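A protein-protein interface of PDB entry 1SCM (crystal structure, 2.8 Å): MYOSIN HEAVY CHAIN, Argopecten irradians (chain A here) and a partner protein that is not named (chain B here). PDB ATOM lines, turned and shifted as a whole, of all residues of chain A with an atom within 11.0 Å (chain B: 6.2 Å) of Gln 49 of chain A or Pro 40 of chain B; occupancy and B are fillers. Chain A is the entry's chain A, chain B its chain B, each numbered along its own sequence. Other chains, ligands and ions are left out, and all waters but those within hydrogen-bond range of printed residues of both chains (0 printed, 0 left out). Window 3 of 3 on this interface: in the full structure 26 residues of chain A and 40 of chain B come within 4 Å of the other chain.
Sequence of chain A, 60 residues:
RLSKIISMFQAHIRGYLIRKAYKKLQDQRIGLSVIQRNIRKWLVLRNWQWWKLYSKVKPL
The side-chain hydroxyl (OG) of Ser 33 of chain B sits at hydrogen-bond distance from the backbone carbonyl oxygen (O) of Ile 29 of chain B.
The side-chain carboxylate (OD1) of Asp 41 of chain B is in hydrogen-bond range of the backbone NH (N) of Glu 44 of chain B (2.9 Å).
Printed residues of chain B that touch a printed residue of chain A: Ile 29, Ser 33, Pro 40, Glu 44 and Met 48.
Along chain B the printed residues that touch a printed residue of chain A span positions 29 to 48.
Hydrophobic or aromatic side chains of chain A within 4 Å of the printed part of chain B: Trp 50 and Leu 53.
Along chain A the printed residues that touch a printed residue of chain B span positions 49 to 53.
Among the printed residues, 7 pairs touch across the chains.
Among the printed residues, no Asp or Glu carboxylate lies within 4 Å of a Lys or Arg side-chain nitrogen of the other chain.
Among the printed residues, pairs that only touch across the chains: Gln 49 of chain A with Glu 44 of chain B (3.5 Å), Gln 49 of chain A with Pro 40 of chain B (3.7 Å), Leu 53 of chain A with Met 48 of chain B (3.8 Å), Gln 49 of chain A with Met 48 of chain B (3.8 Å), Leu 53 of chain A with Ser 33 of chain B (3.8 Å) and Leu 53 of chain A with Ile 29 of chain B (3.9 Å).
The indole nitrogen of Trp 50 of chain A sits close to the backbone carbonyl oxygen of Met 48 of chain B.
Pro 40 of chain B touches one residue of chain A.
Asp 41 of chain B touches none of the printed residues of chain A.
Of chain A, only Gln 49 comes within 4 Å of Glu 44 of chain B.
Of the printed residues of chain B, Trp 50 of chain A touches Met 48.
Of the printed residues of chain A, Met 48 of chain B touches Gln 49, Trp 50 and Leu 53.
Of the printed residues of chain A, Ile 29 of chain B touches Leu 53 (3.9 Å).
Of the printed residues of chain B, Leu 53 of chain A touches Ile 29, Ser 33 and Met 48.
Asp 42 of chain B touches none of the printed residues of chain A.
The nearest residue of chain A that does not touch Pro 40 of chain B is Leu 53 of chain A (7.0 Å).
The nearest printed residue of chain A that does not touch Met 48 of chain B is Trp 51 of chain A (6.4 Å).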
ATOM      1  N   TRP A  42       6.999 -29.985  15.150  1.00  0.00           N
ATOM      2  CA  TRP A  42       7.337 -30.666  13.909  1.00  0.00           C
ATOM      3  C   TRP A  42       6.205 -30.648  12.902  1.00  0.00           C
ATOM      4  O   TRP A  42       6.415 -30.235  11.769  1.00  0.00           O
ATOM      5  CB  TRP A  42       7.714 -32.070  14.287  1.00  0.00           C
ATOM      6  CG  TRP A  42       8.071 -33.037  13.182  1.00  0.00           C
ATOM      7  CD1 TRP A  42       9.196 -32.865  12.414  1.00  0.00           C
ATOM      8  CD2 TRP A  42       7.356 -34.179  12.895  1.00  0.00           C
ATOM      9  NE1 TRP A  42       9.209 -33.930  11.644  1.00  0.00           N
ATOM     10  CE2 TRP A  42       8.144 -34.737  11.881  1.00  0.00           C
ATOM     11  CE3 TRP A  42       6.190 -34.824  13.325  1.00  0.00           C
ATOM     12  CZ2 TRP A  42       7.755 -35.952  11.298  1.00  0.00           C
ATOM     13  CZ3 TRP A  42       5.819 -36.029  12.735  1.00  0.00           C
ATOM     14  CH2 TRP A  42       6.592 -36.593  11.729  1.00  0.00           C
ATOM     15  N   LEU A  43       5.007 -31.099  13.274  1.00  0.00           N
ATOM     16  CA  LEU A  43       3.848 -31.032  12.406  1.00  0.00           C
ATOM     17  C   LEU A  43       3.706 -29.631  11.787  1.00  0.00           C
ATOM     18  O   LEU A  43       3.500 -29.483  10.583  1.00  0.00           O
ATOM     19  CB  LEU A  43       2.676 -31.508  13.321  1.00  0.00           C
ATOM     20  CG  LEU A  43       1.835 -32.853  13.128  1.00  0.00           C
ATOM     21  CD1 LEU A  43       2.691 -33.962  12.513  1.00  0.00           C
ATOM     22  CD2 LEU A  43       1.236 -33.282  14.485  1.00  0.00           C
ATOM     23  N   VAL A  44       3.938 -28.583  12.575  1.00  0.00           N
ATOM     24  CA  VAL A  44       4.019 -27.200  12.072  1.00  0.00           C
ATOM     25  C   VAL A  44       5.060 -26.972  10.976  1.00  0.00           C
ATOM     26  O   VAL A  44       4.695 -26.544   9.894  1.00  0.00           O
ATOM     27  CB  VAL A  44       4.313 -26.199  13.253  1.00  0.00           C
ATOM     28  CG1 VAL A  44       4.634 -24.827  12.725  1.00  0.00           C
ATOM     29  CG2 VAL A  44       3.067 -26.010  14.120  1.00  0.00           C
ATOM     30  N   LEU A  45       6.329 -27.254  11.258  1.00  0.00           N
ATOM     31  CA  LEU A  45       7.452 -27.150  10.326  1.00  0.00           C
ATOM     32  C   LEU A  45       7.199 -27.572   8.899  1.00  0.00           C
ATOM     33  O   LEU A  45       7.369 -26.820   7.935  1.00  0.00           O
ATOM     34  CB  LEU A  45       8.650 -28.001  10.794  1.00  0.00           C
ATOM     35  CG  LEU A  45       9.839 -27.334  11.452  1.00  0.00           C
ATOM     36  CD1 LEU A  45      10.608 -26.599  10.366  1.00  0.00           C
ATOM     37  CD2 LEU A  45       9.372 -26.419  12.613  1.00  0.00           C
ATOM     38  N   ARG A  46       6.756 -28.819   8.849  1.00  0.00           N
ATOM     39  CA  ARG A  46       6.525 -29.542   7.623  1.00  0.00           C
ATOM     40  C   ARG A  46       5.340 -29.019   6.906  1.00  0.00           C
ATOM     41  O   ARG A  46       5.133 -29.469   5.787  1.00  0.00           O
ATOM     42  CB  ARG A  46       6.219 -30.964   7.849  1.00  0.00           C
ATOM     43  CG  ARG A  46       6.957 -31.656   8.951  1.00  0.00           C
ATOM     44  CD  ARG A  46       6.002 -32.775   9.249  1.00  0.00           C
ATOM     45  NE  ARG A  46       6.040 -33.755   8.181  1.00  0.00           N
ATOM     46  CZ  ARG A  46       4.958 -34.109   7.493  1.00  0.00           C
ATOM     47  NH1 ARG A  46       3.754 -33.577   7.735  1.00  0.00           N
ATOM     48  NH2 ARG A  46       5.132 -35.015   6.532  1.00  0.00           N
ATOM     49  N   ASN A  47       4.519 -28.192   7.543  1.00  0.00           N
ATOM     50  CA  ASN A  47       3.443 -27.556   6.819  1.00  0.00           C
ATOM     51  C   ASN A  47       3.732 -26.089   6.496  1.00  0.00           C
ATOM     52  O   ASN A  47       2.880 -25.342   6.019  1.00  0.00           O
ATOM     53  CB  ASN A  47       2.171 -27.711   7.635  1.00  0.00           C
ATOM     54  CG  ASN A  47       1.532 -29.086   7.441  1.00  0.00           C
ATOM     55  OD1 ASN A  47       0.890 -29.338   6.419  1.00  0.00           O
ATOM     56  ND2 ASN A  47       1.667 -30.029   8.381  1.00  0.00           N
ATOM     57  N   TRP A  48       4.973 -25.642   6.679  1.00  0.00           N
ATOM     58  CA  TRP A  48       5.409 -24.268   6.411  1.00  0.00           C
ATOM     59  C   TRP A  48       6.291 -24.320   5.181  1.00  0.00           C
ATOM     60  O   TRP A  48       7.328 -24.991   5.119  1.00  0.00           O
ATOM     61  CB  TRP A  48       6.139 -23.764   7.663  1.00  0.00           C
ATOM     62  CG  TRP A  48       7.116 -22.606   7.566  1.00  0.00           C
ATOM     63  CD1 TRP A  48       6.741 -21.300   7.385  1.00  0.00           C
ATOM     64  CD2 TRP A  48       8.461 -22.731   7.733  1.00  0.00           C
ATOM     65  NE1 TRP A  48       7.851 -20.594   7.462  1.00  0.00           N
ATOM     66  CE2 TRP A  48       8.893 -21.406   7.668  1.00  0.00           C
ATOM     67  CE3 TRP A  48       9.348 -23.772   7.949  1.00  0.00           C
ATOM     68  CZ2 TRP A  48      10.226 -21.096   7.814  1.00  0.00           C
ATOM     69  CZ3 TRP A  48      10.682 -23.461   8.099  1.00  0.00           C
ATOM     70  CH2 TRP A  48      11.112 -22.137   8.026  1.00  0.00           C
ATOM     71  N   GLN A  49       5.827 -23.545   4.209  1.00  0.00           N
ATOM     72  CA  GLN A  49       6.397 -23.623   2.893  1.00  0.00           C
ATOM     73  C   GLN A  49       7.875 -23.386   2.696  1.00  0.00           C
ATOM     74  O   GLN A  49       8.422 -23.962   1.756  1.00  0.00           O
ATOM     75  CB  GLN A  49       5.555 -22.708   2.005  1.00  0.00           C
ATOM     76  CG  GLN A  49       4.403 -23.429   1.249  1.00  0.00           C
ATOM     77  CD  GLN A  49       4.851 -24.367   0.124  1.00  0.00           C
ATOM     78  OE1 GLN A  49       6.043 -24.523  -0.167  1.00  0.00           O
ATOM     79  NE2 GLN A  49       3.937 -25.043  -0.578  1.00  0.00           N
ATOM     80  N   TRP A  50       8.599 -22.616   3.502  1.00  0.00           N
ATOM     81  CA  TRP A  50      10.040 -22.572   3.309  1.00  0.00           C
ATOM     82  C   TRP A  50      10.638 -23.912   3.658  1.00  0.00           C
ATOM     83  O   TRP A  50      11.536 -24.310   2.921  1.00  0.00           O
ATOM     84  CB  TRP A  50      10.756 -21.574   4.179  1.00  0.00           C
ATOM     85  CG  TRP A  50      10.474 -20.135   3.816  1.00  0.00           C
ATOM     86  CD1 TRP A  50       9.592 -19.416   4.566  1.00  0.00           C
ATOM     87  CD2 TRP A  50      11.024 -19.391   2.798  1.00  0.00           C
ATOM     88  NE1 TRP A  50       9.577 -18.213   4.041  1.00  0.00           N
ATOM     89  CE2 TRP A  50      10.406 -18.152   2.996  1.00  0.00           C
ATOM     90  CE3 TRP A  50      11.926 -19.541   1.754  1.00  0.00           C
ATOM     91  CZ2 TRP A  50      10.673 -17.063   2.179  1.00  0.00           C
ATOM     92  CZ3 TRP A  50      12.200 -18.460   0.928  1.00  0.00           C
ATOM     93  CH2 TRP A  50      11.581 -17.235   1.145  1.00  0.00           C
ATOM     94  N   TRP A  51      10.139 -24.621   4.707  1.00  0.00           N
ATOM     95  CA  TRP A  51      10.683 -25.925   5.077  1.00  0.00           C
ATOM     96  C   TRP A  51      10.426 -26.938   3.990  1.00  0.00           C
ATOM     97  O   TRP A  51      11.321 -27.710   3.632  1.00  0.00           O
ATOM     98  CB  TRP A  51      10.089 -26.534   6.370  1.00  0.00           C
ATOM     99  CG  TRP A  51      10.943 -27.738   6.814  1.00  0.00           C
ATOM    100  CD1 TRP A  51      10.452 -29.028   6.856  1.00  0.00           C
ATOM    101  CD2 TRP A  51      12.290 -27.688   7.111  1.00  0.00           C
ATOM    102  NE1 TRP A  51      11.479 -29.786   7.151  1.00  0.00           N
ATOM    103  CE2 TRP A  51      12.587 -29.041   7.307  1.00  0.00           C
ATOM    104  CE3 TRP A  51      13.297 -26.711   7.222  1.00  0.00           C
ATOM    105  CZ2 TRP A  51      13.897 -29.414   7.616  1.00  0.00           C
ATOM    106  CZ3 TRP A  51      14.609 -27.093   7.528  1.00  0.00           C
ATOM    107  CH2 TRP A  51      14.904 -28.439   7.727  1.00  0.00           C
ATOM    108  N   LYS A  52       9.196 -26.926   3.462  1.00  0.00           N
ATOM    109  CA  LYS A  52       8.849 -27.825   2.370  1.00  0.00           C
ATOM    110  C   LYS A  52       9.768 -27.606   1.196  1.00  0.00           C
ATOM    111  O   LYS A  52      10.321 -28.589   0.711  1.00  0.00           O
ATOM    112  CB  LYS A  52       7.415 -27.622   1.916  1.00  0.00           C
ATOM    113  CG  LYS A  52       6.476 -28.377   2.845  1.00  0.00           C
ATOM    114  CD  LYS A  52       5.094 -28.581   2.246  1.00  0.00           C
ATOM    115  CE  LYS A  52       4.325 -27.298   2.087  1.00  0.00           C
ATOM    116  NZ  LYS A  52       4.000 -26.715   3.373  1.00  0.00           N
ATOM    117  N   LEU A  53      10.023 -26.334   0.851  1.00  0.00           N
ATOM    118  CA  LEU A  53      10.955 -26.007  -0.211  1.00  0.00           C
ATOM    119  C   LEU A  53      12.342 -26.547   0.092  1.00  0.00           C
ATOM    120  O   LEU A  53      12.914 -27.232  -0.750  1.00  0.00           O
ATOM    121  CB  LEU A  53      11.062 -24.521  -0.402  1.00  0.00           C
ATOM    122  CG  LEU A  53      12.040 -24.021  -1.455  1.00  0.00           C
ATOM    123  CD1 LEU A  53      11.691 -24.598  -2.809  1.00  0.00           C
ATOM    124  CD2 LEU A  53      12.005 -22.491  -1.469  1.00  0.00           C
ATOM    125  N   TYR A  54      12.886 -26.321   1.287  1.00  0.00           N
ATOM    126  CA  TYR A  54      14.221 -26.784   1.638  1.00  0.00           C
ATOM    127  C   TYR A  54      14.301 -28.301   1.537  1.00  0.00           C
ATOM    128  O   TYR A  54      15.240 -28.811   0.920  1.00  0.00           O
ATOM    129  CB  TYR A  54      14.575 -26.304   3.074  1.00  0.00           C
ATOM    130  CG  TYR A  54      16.008 -26.608   3.495  1.00  0.00           C
ATOM    131  CD1 TYR A  54      17.076 -26.121   2.740  1.00  0.00           C
ATOM    132  CD2 TYR A  54      16.267 -27.428   4.595  1.00  0.00           C
ATOM    133  CE1 TYR A  54      18.384 -26.471   3.088  1.00  0.00           C
ATOM    134  CE2 TYR A  54      17.579 -27.767   4.932  1.00  0.00           C
ATOM    135  CZ  TYR A  54      18.643 -27.291   4.178  1.00  0.00           C
ATOM    136  OH  TYR A  54      19.954 -27.632   4.482  1.00  0.00           O
ATOM    137  N   SER A  55      13.267 -29.025   1.993  1.00  0.00           N
ATOM    138  CA  SER A  55      13.318 -30.474   2.009  1.00  0.00           C
ATOM    139  C   SER A  55      13.423 -31.114   0.661  1.00  0.00           C
ATOM    140  O   SER A  55      13.856 -32.257   0.582  1.00  0.00           O
ATOM    141  CB  SER A  55      12.100 -31.013   2.686  1.00  0.00           C
ATOM    142  OG  SER A  55      12.140 -30.761   4.086  1.00  0.00           O
ATOM    143  N   LYS A  56      13.031 -30.346  -0.365  1.00  0.00           N
ATOM    144  CA  LYS A  56      13.031 -30.788  -1.749  1.00  0.00           C
ATOM    145  C   LYS A  56      14.420 -30.602  -2.315  1.00  0.00           C
ATOM    146  O   LYS A  56      14.943 -31.490  -2.978  1.00  0.00           O
ATOM    147  CB  LYS A  56      12.033 -29.984  -2.606  1.00  0.00           C
ATOM    148  CG  LYS A  56      10.522 -29.871  -2.244  1.00  0.00           C
ATOM    149  CD  LYS A  56       9.531 -31.022  -2.542  1.00  0.00           C
ATOM    150  CE  LYS A  56       9.395 -32.096  -1.438  1.00  0.00           C
ATOM    151  NZ  LYS A  56      10.373 -33.185  -1.477  1.00  0.00           N
ATOM    152  N   VAL A  57      15.056 -29.463  -2.058  1.00  0.00           N
ATOM    153  CA  VAL A  57      16.435 -29.176  -2.468  1.00  0.00           C
ATOM    154  C   VAL A  57      17.459 -30.012  -1.646  1.00  0.00           C
ATOM    155  O   VAL A  57      18.605 -30.199  -2.057  1.00  0.00           O
ATOM    156  CB  VAL A  57      16.722 -27.665  -2.253  1.00  0.00           C
ATOM    157  CG1 VAL A  57      18.000 -27.342  -2.993  1.00  0.00           C
ATOM    158  CG2 VAL A  57      15.604 -26.767  -2.749  1.00  0.00           C
ATOM    159  N   ILE B  29      11.612 -18.417  -6.439  1.00  0.00           N
ATOM    160  CA  ILE B  29      10.930 -19.425  -5.657  1.00  0.00           C
ATOM    161  C   ILE B  29      10.044 -20.179  -6.654  1.00  0.00           C
ATOM    162  O   ILE B  29      10.057 -21.401  -6.682  1.00  0.00           O
ATOM    163  CB  ILE B  29      10.030 -18.816  -4.533  1.00  0.00           C
ATOM    164  CG1 ILE B  29      10.610 -17.646  -3.768  1.00  0.00           C
ATOM    165  CG2 ILE B  29       9.882 -19.933  -3.522  1.00  0.00           C
ATOM    166  CD1 ILE B  29       9.569 -17.090  -2.784  1.00  0.00           C
ATOM    167  N   LYS B  30       9.349 -19.474  -7.564  1.00  0.00           N
ATOM    168  CA  LYS B  30       8.497 -20.118  -8.543  1.00  0.00           C
ATOM    169  C   LYS B  30       9.364 -20.959  -9.434  1.00  0.00           C
ATOM    170  O   LYS B  30       9.133 -22.160  -9.516  1.00  0.00           O
ATOM    171  CB  LYS B  30       7.740 -19.071  -9.372  1.00  0.00           C
ATOM    172  CG  LYS B  30       6.721 -19.646 -10.391  1.00  0.00           C
ATOM    173  CD  LYS B  30       5.589 -18.668 -10.733  1.00  0.00           C
ATOM    174  CE  LYS B  30       4.526 -18.649  -9.612  1.00  0.00           C
ATOM    175  NZ  LYS B  30       3.534 -17.594  -9.751  1.00  0.00           N
ATOM    176  N   SER B  33      10.701 -24.042  -7.709  1.00  0.00           N
ATOM    177  CA  SER B  33       9.552 -24.869  -7.390  1.00  0.00           C
ATOM    178  C   SER B  33       8.906 -25.591  -8.570  1.00  0.00           C
ATOM    179  O   SER B  33       8.429 -26.705  -8.367  1.00  0.00           O
ATOM    180  CB  SER B  33       8.576 -23.965  -6.698  1.00  0.00           C
ATOM    181  OG  SER B  33       9.338 -23.445  -5.618  1.00  0.00           O
ATOM    182  N   ARG B  38       5.403 -29.753  -8.275  1.00  0.00           N
ATOM    183  CA  ARG B  38       4.230 -28.919  -8.437  1.00  0.00           C
ATOM    184  C   ARG B  38       4.485 -27.707  -7.571  1.00  0.00           C
ATOM    185  O   ARG B  38       4.801 -27.818  -6.378  1.00  0.00           O
ATOM    186  CB  ARG B  38       2.964 -29.684  -7.976  1.00  0.00           C
ATOM    187  CG  ARG B  38       1.638 -28.894  -8.063  1.00  0.00           C
ATOM    188  CD  ARG B  38       0.341 -29.711  -8.008  1.00  0.00           C
ATOM    189  NE  ARG B  38       0.003 -30.457  -9.224  1.00  0.00           N
ATOM    190  CZ  ARG B  38       0.189 -31.774  -9.305  1.00  0.00           C
ATOM    191  NH1 ARG B  38       0.709 -32.408  -8.267  1.00  0.00           N
ATOM    192  NH2 ARG B  38      -0.216 -32.460 -10.376  1.00  0.00           N
ATOM    193  N   ALA B  39       4.431 -26.553  -8.228  1.00  0.00           N
ATOM    194  CA  ALA B  39       4.659 -25.313  -7.523  1.00  0.00           C
ATOM    195  C   ALA B  39       3.504 -24.998  -6.590  1.00  0.00           C
ATOM    196  O   ALA B  39       2.369 -25.429  -6.857  1.00  0.00           O
ATOM    197  CB  ALA B  39       4.784 -24.180  -8.488  1.00  0.00           C
ATOM    198  N   PRO B  40       3.748 -24.258  -5.480  1.00  0.00           N
ATOM    199  CA  PRO B  40       2.746 -23.431  -4.804  1.00  0.00           C
ATOM    200  C   PRO B  40       2.279 -22.324  -5.739  1.00  0.00           C
ATOM    201  O   PRO B  40       2.757 -22.255  -6.872  1.00  0.00           O
ATOM    202  CB  PRO B  40       3.475 -22.957  -3.579  1.00  0.00           C
ATOM    203  CG  PRO B  40       4.916 -22.937  -4.014  1.00  0.00           C
ATOM    204  CD  PRO B  40       4.991 -24.256  -4.717  1.00  0.00           C
ATOM    205  N   ASP B  41       1.461 -21.363  -5.325  1.00  0.00           N
ATOM    206  CA  ASP B  41       0.875 -20.456  -6.311  1.00  0.00           C
ATOM    207  C   ASP B  41       1.164 -18.950  -6.380  1.00  0.00           C
ATOM    208  O   ASP B  41       1.938 -18.472  -7.219  1.00  0.00           O
ATOM    209  CB  ASP B  41      -0.634 -20.714  -6.241  1.00  0.00           C
ATOM    210  CG  ASP B  41      -1.198 -20.828  -4.833  1.00  0.00           C
ATOM    211  OD1 ASP B  41      -0.785 -20.065  -3.963  1.00  0.00           O
ATOM    212  OD2 ASP B  41      -2.038 -21.696  -4.614  1.00  0.00           O
ATOM    213  N   ASP B  42       0.435 -18.165  -5.596  1.00  0.00           N
ATOM    214  CA  ASP B  42       0.698 -16.764  -5.443  1.00  0.00           C
ATOM    215  C   ASP B  42       0.200 -16.581  -4.032  1.00  0.00           C
ATOM    216  O   ASP B  42       1.019 -16.198  -3.215  1.00  0.00           O
ATOM    217  CB  ASP B  42      -0.085 -15.977  -6.469  1.00  0.00           C
ATOM    218  CG  ASP B  42       0.865 -15.083  -7.260  1.00  0.00           C
ATOM    219  OD1 ASP B  42       1.589 -15.563  -8.139  1.00  0.00           O
ATOM    220  OD2 ASP B  42       0.883 -13.890  -6.972  1.00  0.00           O
ATOM    221  N   GLU B  44       0.300 -18.412  -1.788  1.00  0.00           N
ATOM    222  CA  GLU B  44       1.382 -18.986  -1.027  1.00  0.00           C
ATOM    223  C   GLU B  44       2.710 -18.282  -1.183  1.00  0.00           C
ATOM    224  O   GLU B  44       3.318 -17.904  -0.189  1.00  0.00           O
ATOM    225  CB  GLU B  44       1.580 -20.428  -1.430  1.00  0.00           C
ATOM    226  CG  GLU B  44       0.455 -21.376  -1.086  1.00  0.00           C
ATOM    227  CD  GLU B  44       0.323 -21.542   0.417  1.00  0.00           C
ATOM    228  OE1 GLU B  44       1.028 -22.386   0.983  1.00  0.00           O
ATOM    229  OE2 GLU B  44      -0.471 -20.814   1.015  1.00  0.00           O
ATOM    230  N   LEU B  45       3.118 -18.105  -2.452  1.00  0.00           N
ATOM    231  CA  LEU B  45       4.439 -17.623  -2.835  1.00  0.00           C
ATOM    232  C   LEU B  45       4.682 -16.206  -2.437  1.00  0.00           C
ATOM    233  O   LEU B  45       5.788 -15.891  -2.016  1.00  0.00           O
ATOM    234  CB  LEU B  45       4.610 -17.807  -4.340  1.00  0.00           C
ATOM    235  CG  LEU B  45       4.834 -19.283  -4.721  1.00  0.00           C
ATOM    236  CD1 LEU B  45       4.798 -19.534  -6.203  1.00  0.00           C
ATOM    237  CD2 LEU B  45       6.217 -19.664  -4.260  1.00  0.00           C
ATOM    238  N   MET B  48       5.167 -16.388   1.311  1.00  0.00           N
ATOM    239  CA  MET B  48       6.474 -16.831   1.771  1.00  0.00           C
ATOM    240  C   MET B  48       7.403 -15.669   1.996  1.00  0.00           C
ATOM    241  O   MET B  48       7.970 -15.578   3.083  1.00  0.00           O
ATOM    242  CB  MET B  48       7.143 -17.733   0.777  1.00  0.00           C
ATOM    243  CG  MET B  48       6.817 -19.180   1.013  1.00  0.00           C
ATOM    244  SD  MET B  48       7.261 -20.255  -0.391  1.00  0.00           S
ATOM    245  CE  MET B  48       8.971 -20.670  -0.178  1.00  0.00           C
